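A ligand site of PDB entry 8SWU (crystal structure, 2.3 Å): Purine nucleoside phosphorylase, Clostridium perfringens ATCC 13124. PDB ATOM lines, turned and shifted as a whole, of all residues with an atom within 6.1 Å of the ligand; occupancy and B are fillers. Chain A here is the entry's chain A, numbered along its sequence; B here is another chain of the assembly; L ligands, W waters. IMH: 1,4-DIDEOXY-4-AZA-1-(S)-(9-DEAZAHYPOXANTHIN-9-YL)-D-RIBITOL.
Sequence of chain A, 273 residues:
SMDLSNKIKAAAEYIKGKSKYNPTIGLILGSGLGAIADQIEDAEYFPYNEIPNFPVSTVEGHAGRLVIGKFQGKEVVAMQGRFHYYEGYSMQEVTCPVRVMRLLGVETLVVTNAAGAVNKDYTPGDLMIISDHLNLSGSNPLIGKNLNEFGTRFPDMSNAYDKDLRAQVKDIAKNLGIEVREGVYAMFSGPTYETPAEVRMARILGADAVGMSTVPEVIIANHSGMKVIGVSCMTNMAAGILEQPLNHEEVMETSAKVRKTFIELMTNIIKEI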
ATOM      1  N   HIS A  84       3.353  17.688 -10.311  1.00  0.00           N
ATOM      2  CA  HIS A  84       3.977  18.657  -9.420  1.00  0.00           C
ATOM      3  C   HIS A  84       5.444  18.855  -9.757  1.00  0.00           C
ATOM      4  O   HIS A  84       6.129  17.932 -10.204  1.00  0.00           O
ATOM      5  CB  HIS A  84       3.831  18.233  -7.950  1.00  0.00           C
ATOM      6  CG  HIS A  84       2.415  18.067  -7.500  1.00  0.00           C
ATOM      7  ND1 HIS A  84       1.651  16.963  -7.829  1.00  0.00           N
ATOM      8  CD2 HIS A  84       1.622  18.860  -6.738  1.00  0.00           C
ATOM      9  CE1 HIS A  84       0.450  17.095  -7.288  1.00  0.00           C
ATOM     10  NE2 HIS A  84       0.409  18.233  -6.624  1.00  0.00           N
ATOM     11  N   TYR A  86       7.756  19.303  -7.575  1.00  0.00           N
ATOM     12  CA  TYR A  86       8.607  18.641  -6.589  1.00  0.00           C
ATOM     13  C   TYR A  86       8.915  17.189  -6.946  1.00  0.00           C
ATOM     14  O   TYR A  86       9.818  16.611  -6.337  1.00  0.00           O
ATOM     15  CB  TYR A  86       7.978  18.704  -5.192  1.00  0.00           C
ATOM     16  CG  TYR A  86       6.588  18.115  -5.035  1.00  0.00           C
ATOM     17  CD1 TYR A  86       6.355  16.748  -5.178  1.00  0.00           C
ATOM     18  CD2 TYR A  86       5.505  18.924  -4.723  1.00  0.00           C
ATOM     19  CE1 TYR A  86       5.082  16.216  -5.040  1.00  0.00           C
ATOM     20  CE2 TYR A  86       4.239  18.404  -4.568  1.00  0.00           C
ATOM     21  CZ  TYR A  86       4.027  17.047  -4.733  1.00  0.00           C
ATOM     22  OH  TYR A  86       2.760  16.527  -4.578  1.00  0.00           O
ATOM     23  N   ALA A 114      -4.819  21.995  -2.489  1.00  0.00           N
ATOM     24  CA  ALA A 114      -4.735  21.952  -1.037  1.00  0.00           C
ATOM     25  C   ALA A 114      -3.558  22.817  -0.587  1.00  0.00           C
ATOM     26  O   ALA A 114      -2.507  22.818  -1.230  1.00  0.00           O
ATOM     27  CB  ALA A 114      -4.556  20.518  -0.529  1.00  0.00           C
ATOM     28  N   ALA A 115      -3.757  23.556   0.504  1.00  0.00           N
ATOM     29  CA  ALA A 115      -2.741  24.500   0.954  1.00  0.00           C
ATOM     30  C   ALA A 115      -2.831  24.672   2.462  1.00  0.00           C
ATOM     31  O   ALA A 115      -3.858  24.376   3.081  1.00  0.00           O
ATOM     32  CB  ALA A 115      -2.895  25.856   0.254  1.00  0.00           C
ATOM     33  N   GLY A 116      -1.733  25.151   3.039  1.00  0.00           N
ATOM     34  CA  GLY A 116      -1.700  25.480   4.451  1.00  0.00           C
ATOM     35  C   GLY A 116      -2.068  26.937   4.671  1.00  0.00           C
ATOM     36  O   GLY A 116      -1.615  27.821   3.941  1.00  0.00           O
ATOM     37  N   ALA A 117      -2.897  27.176   5.678  1.00  0.00           N
ATOM     38  CA  ALA A 117      -3.399  28.522   5.958  1.00  0.00           C
ATOM     39  C   ALA A 117      -2.342  29.332   6.692  1.00  0.00           C
ATOM     40  O   ALA A 117      -1.951  28.993   7.817  1.00  0.00           O
ATOM     41  CB  ALA A 117      -4.682  28.442   6.795  1.00  0.00           C
ATOM     42  N   TYR A 185      -2.178  33.299  -2.590  1.00  0.00           N
ATOM     43  CA  TYR A 185      -1.614  31.963  -2.475  1.00  0.00           C
ATOM     44  C   TYR A 185      -0.140  31.999  -2.887  1.00  0.00           C
ATOM     45  O   TYR A 185       0.180  32.474  -3.974  1.00  0.00           O
ATOM     46  CB  TYR A 185      -2.396  30.972  -3.343  1.00  0.00           C
ATOM     47  CG  TYR A 185      -1.736  29.625  -3.558  1.00  0.00           C
ATOM     48  CD1 TYR A 185      -0.843  29.434  -4.592  1.00  0.00           C
ATOM     49  CD2 TYR A 185      -2.025  28.551  -2.725  1.00  0.00           C
ATOM     50  CE1 TYR A 185      -0.241  28.205  -4.800  1.00  0.00           C
ATOM     51  CE2 TYR A 185      -1.432  27.321  -2.916  1.00  0.00           C
ATOM     52  CZ  TYR A 185      -0.541  27.152  -3.960  1.00  0.00           C
ATOM     53  OH  TYR A 185       0.061  25.937  -4.167  1.00  0.00           O
ATOM     54  N   THR A 192       9.390  19.491   0.743  1.00  0.00           N
ATOM     55  CA  THR A 192       9.411  19.746   2.173  1.00  0.00           C
ATOM     56  C   THR A 192       8.239  20.643   2.561  1.00  0.00           C
ATOM     57  O   THR A 192       7.830  21.525   1.807  1.00  0.00           O
ATOM     58  CB  THR A 192      10.721  20.422   2.582  1.00  0.00           C
ATOM     59  OG1 THR A 192      11.125  21.349   1.565  1.00  0.00           O
ATOM     60  CG2 THR A 192      11.819  19.390   2.783  1.00  0.00           C
ATOM     61  N   TYR A 193       7.696  20.411   3.750  1.00  0.00           N
ATOM     62  CA  TYR A 193       6.825  21.410   4.356  1.00  0.00           C
ATOM     63  C   TYR A 193       7.670  22.587   4.832  1.00  0.00           C
ATOM     64  O   TYR A 193       8.823  22.424   5.243  1.00  0.00           O
ATOM     65  CB  TYR A 193       6.042  20.816   5.525  1.00  0.00           C
ATOM     66  CG  TYR A 193       4.937  19.877   5.118  1.00  0.00           C
ATOM     67  CD1 TYR A 193       3.888  20.321   4.316  1.00  0.00           C
ATOM     68  CD2 TYR A 193       4.932  18.547   5.523  1.00  0.00           C
ATOM     69  CE1 TYR A 193       2.870  19.460   3.944  1.00  0.00           C
ATOM     70  CE2 TYR A 193       3.914  17.686   5.152  1.00  0.00           C
ATOM     71  CZ  TYR A 193       2.894  18.144   4.357  1.00  0.00           C
ATOM     72  OH  TYR A 193       1.882  17.290   3.989  1.00  0.00           O
ATOM     73  N   GLU A 194       7.086  23.777   4.746  1.00  0.00           N
ATOM     74  CA  GLU A 194       7.835  24.985   5.091  1.00  0.00           C
ATOM     75  C   GLU A 194       8.256  24.954   6.549  1.00  0.00           C
ATOM     76  O   GLU A 194       7.603  24.356   7.399  1.00  0.00           O
ATOM     77  CB  GLU A 194       6.985  26.227   4.816  1.00  0.00           C
ATOM     78  CG  GLU A 194       6.579  26.423   3.352  1.00  0.00           C
ATOM     79  CD  GLU A 194       5.496  25.453   2.918  1.00  0.00           C
ATOM     80  OE1 GLU A 194       4.632  25.105   3.749  1.00  0.00           O
ATOM     81  OE2 GLU A 194       5.515  25.023   1.742  1.00  0.00           O
ATOM     82  N   VAL A 210      -0.008  28.763   1.664  1.00  0.00           N
ATOM     83  CA  VAL A 210       1.195  28.212   1.048  1.00  0.00           C
ATOM     84  C   VAL A 210       0.881  26.828   0.499  1.00  0.00           C
ATOM     85  O   VAL A 210       0.214  26.015   1.151  1.00  0.00           O
ATOM     86  CB  VAL A 210       2.362  28.150   2.057  1.00  0.00           C
ATOM     87  CG1 VAL A 210       2.924  29.546   2.309  1.00  0.00           C
ATOM     88  CG2 VAL A 210       1.920  27.505   3.355  1.00  0.00           C
ATOM     89  N   GLY A 211       1.377  26.562  -0.711  1.00  0.00           N
ATOM     90  CA  GLY A 211       1.188  25.278  -1.362  1.00  0.00           C
ATOM     91  C   GLY A 211       2.358  24.986  -2.286  1.00  0.00           C
ATOM     92  O   GLY A 211       3.311  25.751  -2.379  1.00  0.00           O
ATOM     93  N   MET A 212       2.272  23.870  -2.997  1.00  0.00           N
ATOM     94  CA  MET A 212       3.382  23.457  -3.878  1.00  0.00           C
ATOM     95  C   MET A 212       2.894  23.335  -5.324  1.00  0.00           C
ATOM     96  O   MET A 212       3.528  22.599  -6.076  1.00  0.00           O
ATOM     97  CB  MET A 212       3.969  22.116  -3.428  1.00  0.00           C
ATOM     98  CG  MET A 212       4.536  22.068  -2.028  1.00  0.00           C
ATOM     99  SD  MET A 212       4.859  20.358  -1.555  1.00  0.00           S
ATOM    100  CE  MET A 212       4.996  20.502   0.228  1.00  0.00           C
ATOM    101  N   SER A 213       1.821  24.028  -5.669  1.00  0.00           N
ATOM    102  CA  SER A 213       1.237  23.907  -7.031  1.00  0.00           C
ATOM    103  C   SER A 213       0.578  25.194  -7.528  1.00  0.00           C
ATOM    104  O   SER A 213       1.061  26.258  -7.120  1.00  0.00           O
ATOM    105  CB  SER A 213       0.203  22.808  -7.037  1.00  0.00           C
ATOM    106  OG  SER A 213      -1.028  23.223  -6.490  1.00  0.00           O
ATOM    107  N   THR A 235      -6.337  22.947   4.192  1.00  0.00           N
ATOM    108  CA  THR A 235      -6.294  21.620   4.787  1.00  0.00           C
ATOM    109  C   THR A 235      -5.549  21.579   6.116  1.00  0.00           C
ATOM    110  O   THR A 235      -5.660  20.580   6.839  1.00  0.00           O
ATOM    111  CB  THR A 235      -5.658  20.622   3.818  1.00  0.00           C
ATOM    112  OG1 THR A 235      -4.305  21.016   3.534  1.00  0.00           O
ATOM    113  CG2 THR A 235      -6.452  20.550   2.529  1.00  0.00           C
ATOM    114  N   ASN A 236      -4.816  22.631   6.455  1.00  0.00           N
ATOM    115  CA  ASN A 236      -4.056  22.694   7.689  1.00  0.00           C
ATOM    116  C   ASN A 236      -3.627  24.130   7.917  1.00  0.00           C
ATOM    117  O   ASN A 236      -3.556  24.929   6.984  1.00  0.00           O
ATOM    118  CB  ASN A 236      -2.821  21.786   7.635  1.00  0.00           C
ATOM    119  CG  ASN A 236      -1.958  22.054   6.412  1.00  0.00           C
ATOM    120  OD1 ASN A 236      -2.281  21.639   5.311  1.00  0.00           O
ATOM    121  ND2 ASN A 236      -0.850  22.751   6.618  1.00  0.00           N
ATOM    122  N   MET A 237      -3.353  24.449   9.175  1.00  0.00           N
ATOM    123  CA  MET A 237      -2.655  25.687   9.495  1.00  0.00           C
ATOM    124  C   MET A 237      -1.181  25.521   9.174  1.00  0.00           C
ATOM    125  O   MET A 237      -0.589  24.474   9.468  1.00  0.00           O
ATOM    126  CB  MET A 237      -2.858  26.073  10.954  1.00  0.00           C
ATOM    127  CG  MET A 237      -4.294  25.963  11.412  1.00  0.00           C
ATOM    128  SD  MET A 237      -5.335  27.216  10.626  1.00  0.00           S
ATOM    129  CE  MET A 237      -4.305  28.671  10.768  1.00  0.00           C
ATOM    130  N   ALA A 238      -0.590  26.541   8.551  1.00  0.00           N
ATOM    131  CA  ALA A 238       0.780  26.450   8.088  1.00  0.00           C
ATOM    132  C   ALA A 238       1.729  26.165   9.246  1.00  0.00           C
ATOM    133  O   ALA A 238       1.411  26.392  10.413  1.00  0.00           O
ATOM    134  CB  ALA A 238       1.173  27.744   7.365  1.00  0.00           C
ATOM    135  N   ALA A 239       2.916  25.662   8.905  1.00  0.00           N
ATOM    136  CA  ALA A 239       3.842  25.172   9.909  1.00  0.00           C
ATOM    137  C   ALA A 239       4.257  26.274  10.872  1.00  0.00           C
ATOM    138  O   ALA A 239       4.487  27.421  10.477  1.00  0.00           O
ATOM    139  CB  ALA A 239       5.082  24.578   9.239  1.00  0.00           C
ATOM    140  N   LEU A 246       3.485  18.736  10.692  1.00  0.00           N
ATOM    141  CA  LEU A 246       2.631  18.713   9.525  1.00  0.00           C
ATOM    142  C   LEU A 246       2.700  17.348   8.860  1.00  0.00           C
ATOM    143  O   LEU A 246       3.780  16.774   8.692  1.00  0.00           O
ATOM    144  CB  LEU A 246       3.024  19.807   8.535  1.00  0.00           C
ATOM    145  CG  LEU A 246       2.271  21.125   8.785  1.00  0.00           C
ATOM    146  CD1 LEU A 246       2.608  22.174   7.734  1.00  0.00           C
ATOM    147  CD2 LEU A 246       0.773  20.863   8.842  1.00  0.00           C
ATOM    148  N   ASN A 247       1.528  16.815   8.500  1.00  0.00           N
ATOM    149  CA  ASN A 247       1.401  15.433   8.068  1.00  0.00           C
ATOM    150  C   ASN A 247       0.474  15.383   6.857  1.00  0.00           C
ATOM    151  O   ASN A 247      -0.610  15.986   6.888  1.00  0.00           O
ATOM    152  CB  ASN A 247       0.847  14.567   9.194  1.00  0.00           C
ATOM    153  CG  ASN A 247       1.138  13.090   8.997  1.00  0.00           C
ATOM    154  OD1 ASN A 247       0.989  12.553   7.897  1.00  0.00           O
ATOM    155  ND2 ASN A 247       1.545  12.424  10.066  1.00  0.00           N
ATOM    156  N   HIS A 248       0.878  14.685   5.794  1.00  0.00           N
ATOM    157  CA  HIS A 248       0.056  14.564   4.553  1.00  0.00           C
ATOM    158  C   HIS A 248      -1.276  13.831   4.817  1.00  0.00           C
ATOM    159  O   HIS A 248      -2.248  14.089   4.116  1.00  0.00           O
ATOM    160  CB  HIS A 248       0.835  13.941   3.388  1.00  0.00           C
ATOM    161  CG  HIS A 248       0.056  13.946   2.117  1.00  0.00           C
ATOM    162  ND1 HIS A 248      -0.413  15.106   1.538  1.00  0.00           N
ATOM    163  CD2 HIS A 248      -0.368  12.951   1.347  1.00  0.00           C
ATOM    164  CE1 HIS A 248      -1.078  14.805   0.443  1.00  0.00           C
ATOM    165  NE2 HIS A 248      -1.069  13.504   0.306  1.00  0.00           N
ATOM    166  N   VAL A 251      -3.775  16.461   5.624  1.00  0.00           N
ATOM    167  CA  VAL A 251      -4.212  17.179   4.393  1.00  0.00           C
ATOM    168  C   VAL A 251      -5.336  16.372   3.749  1.00  0.00           C
ATOM    169  O   VAL A 251      -6.389  16.956   3.437  1.00  0.00           O
ATOM    170  CB  VAL A 251      -3.012  17.404   3.436  1.00  0.00           C
ATOM    171  CG1 VAL A 251      -3.457  17.818   2.047  1.00  0.00           C
ATOM    172  CG2 VAL A 251      -2.009  18.385   4.011  1.00  0.00           C
ATOM    173  N   PHE B 154       6.540  13.886   1.923  1.00  0.00           N
ATOM    174  CA  PHE B 154       6.345  15.247   2.436  1.00  0.00           C
ATOM    175  C   PHE B 154       6.875  15.302   3.863  1.00  0.00           C
ATOM    176  O   PHE B 154       6.098  15.235   4.825  1.00  0.00           O
ATOM    177  CB  PHE B 154       4.879  15.653   2.376  1.00  0.00           C
ATOM    178  CG  PHE B 154       4.285  15.590   1.005  1.00  0.00           C
ATOM    179  CD1 PHE B 154       4.712  16.445   0.003  1.00  0.00           C
ATOM    180  CD2 PHE B 154       3.296  14.659   0.709  1.00  0.00           C
ATOM    181  CE1 PHE B 154       4.164  16.380  -1.262  1.00  0.00           C
ATOM    182  CE2 PHE B 154       2.747  14.594  -0.556  1.00  0.00           C
ATOM    183  CZ  PHE B 154       3.182  15.447  -1.542  1.00  0.00           C
HETATM  184  O5' IMH L   1       0.389  17.486   1.600  1.00  0.00           O
HETATM  185  C5' IMH L   1       1.246  18.001   0.600  1.00  0.00           C
HETATM  186  C4' IMH L   1       0.500  18.237  -0.692  1.00  0.00           C
HETATM  187  N4' IMH L   1      -0.672  19.103  -0.492  1.00  0.00           N
HETATM  188  C3' IMH L   1       1.321  18.991  -1.750  1.00  0.00           C
HETATM  189  O3' IMH L   1       0.951  18.619  -3.069  1.00  0.00           O
HETATM  190  C2' IMH L   1       1.033  20.462  -1.426  1.00  0.00           C
HETATM  191  O2' IMH L   1       0.859  21.261  -2.589  1.00  0.00           O
HETATM  192  C1' IMH L   1      -0.282  20.511  -0.613  1.00  0.00           C
HETATM  193  C9  IMH L   1      -0.225  21.175   0.739  1.00  0.00           C
HETATM  194  C8  IMH L   1      -1.202  21.116   1.682  1.00  0.00           C
HETATM  195  N7  IMH L   1      -0.813  21.827   2.778  1.00  0.00           N
HETATM  196  C5  IMH L   1       0.432  22.348   2.530  1.00  0.00           C
HETATM  197  C6  IMH L   1       1.332  23.153   3.256  1.00  0.00           C
HETATM  198  O6  IMH L   1       1.033  23.574   4.481  1.00  0.00           O
HETATM  199  N1  IMH L   1       2.480  23.503   2.712  1.00  0.00           N
HETATM  200  C2  IMH L   1       2.754  23.068   1.471  1.00  0.00           C
HETATM  201  N3  IMH L   1       2.000  22.315   0.719  1.00  0.00           N
HETATM  202  C4  IMH L   1       0.817  21.957   1.253  1.00  0.00           C
HETATM  203  O   HOH W   1       3.060  24.928   5.935  1.00  0.00           O
HETATM  204  O   HOH W   2      -2.977  17.025  -1.653  1.00  0.00           O
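A ring nitrogen (ND1) of His 248 sits at hydrogen-bond distance from an oxygen (O5') of the ligand (2.5 Å). An oxygen (O5') of the ligand sits at hydrogen-bond distance from the side-chain hydroxyl (OH) of Tyr 193, 2.8 Å away. N1 of the ligand lies within hydrogen-bond range of OE1 of Glu 194 (2.9 Å). A nitrogen (N7) of the ligand lies within hydrogen-bond range of the side-chain amide oxygen of Asn 236, at 2.9 Å. An oxygen (O2') of the ligand lies within hydrogen-bond range of the backbone NH (N) of Met 212. The side-chain hydroxyl of Tyr 86 is in hydrogen-bond range of an oxygen (O3') of the ligand (3.2 Å). The backbone NH (N) of Gly 116 lies close to an oxygen (O6) of the ligand, at 3.5 Å.
Water W1 lies within hydrogen-bond range of the side-chain carboxylate (OE1) of Glu 194 (2.7 Å), an oxygen (O6) of the ligand (2.8 Å) and the backbone NH (N) of Ala 239 (3.1 Å).
The backbone NH (N) of His 248 is in hydrogen-bond range of the side-chain hydroxyl (OH) of Tyr 193. The backbone NH (N) of Gly 116 is in hydrogen-bond range of the backbone carbonyl oxygen (O) of Val 210 (2.8 Å). The side-chain amide oxygen of Asn 236 lies within hydrogen-bond range of the side-chain hydroxyl of Thr 235, 2.8 Å away. The backbone NH (N) of Met 212 sits at hydrogen-bond distance from the side-chain hydroxyl (OH) of Tyr 185. The backbone carbonyl oxygen (O) of Asn 236 sits at hydrogen-bond distance from the backbone NH (N) of Ala 117 (2.7 Å). The backbone carbonyl oxygen (O) of Ala 115 sits at hydrogen-bond distance from the backbone NH (N) of Thr 235 (3.1 Å). The side-chain hydroxyl (OH) of Tyr 86 sits close to a ring nitrogen (ND1) of His 84 (3.5 Å).
His 84 touches the ligand (NE2 to O3', 3.6 Å). O of Ala 114 touches C1' of the ligand (3.3 Å). Ala 115 touches the ligand. O of Val 210 touches C6 of the ligand (3.7 Å). Gly 211 touches the ligand. Thr 235 touches the ligand. CD1 of Leu 246 touches O6 of the ligand, 3.9 Å away. CG2 of Val 251 touches O5' of the ligand, 3.5 Å away. Phe 154 of chain B touches the ligand. Hydrophobic or aromatic side chains within 4 Å of the ligand: His 84, Tyr 86, Tyr 193, Met 212, Leu 246, His 248, Val 251 and Phe 154 of chain B. 16 residues have an atom within 4 Å of the ligand: His 84, Tyr 86, Ala 114, Ala 115, Gly 116, Tyr 193, Glu 194, Val 210, Gly 211, Met 212, Thr 235, Asn 236, Leu 246, His 248, Val 251 and Phe 154 of chain B.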
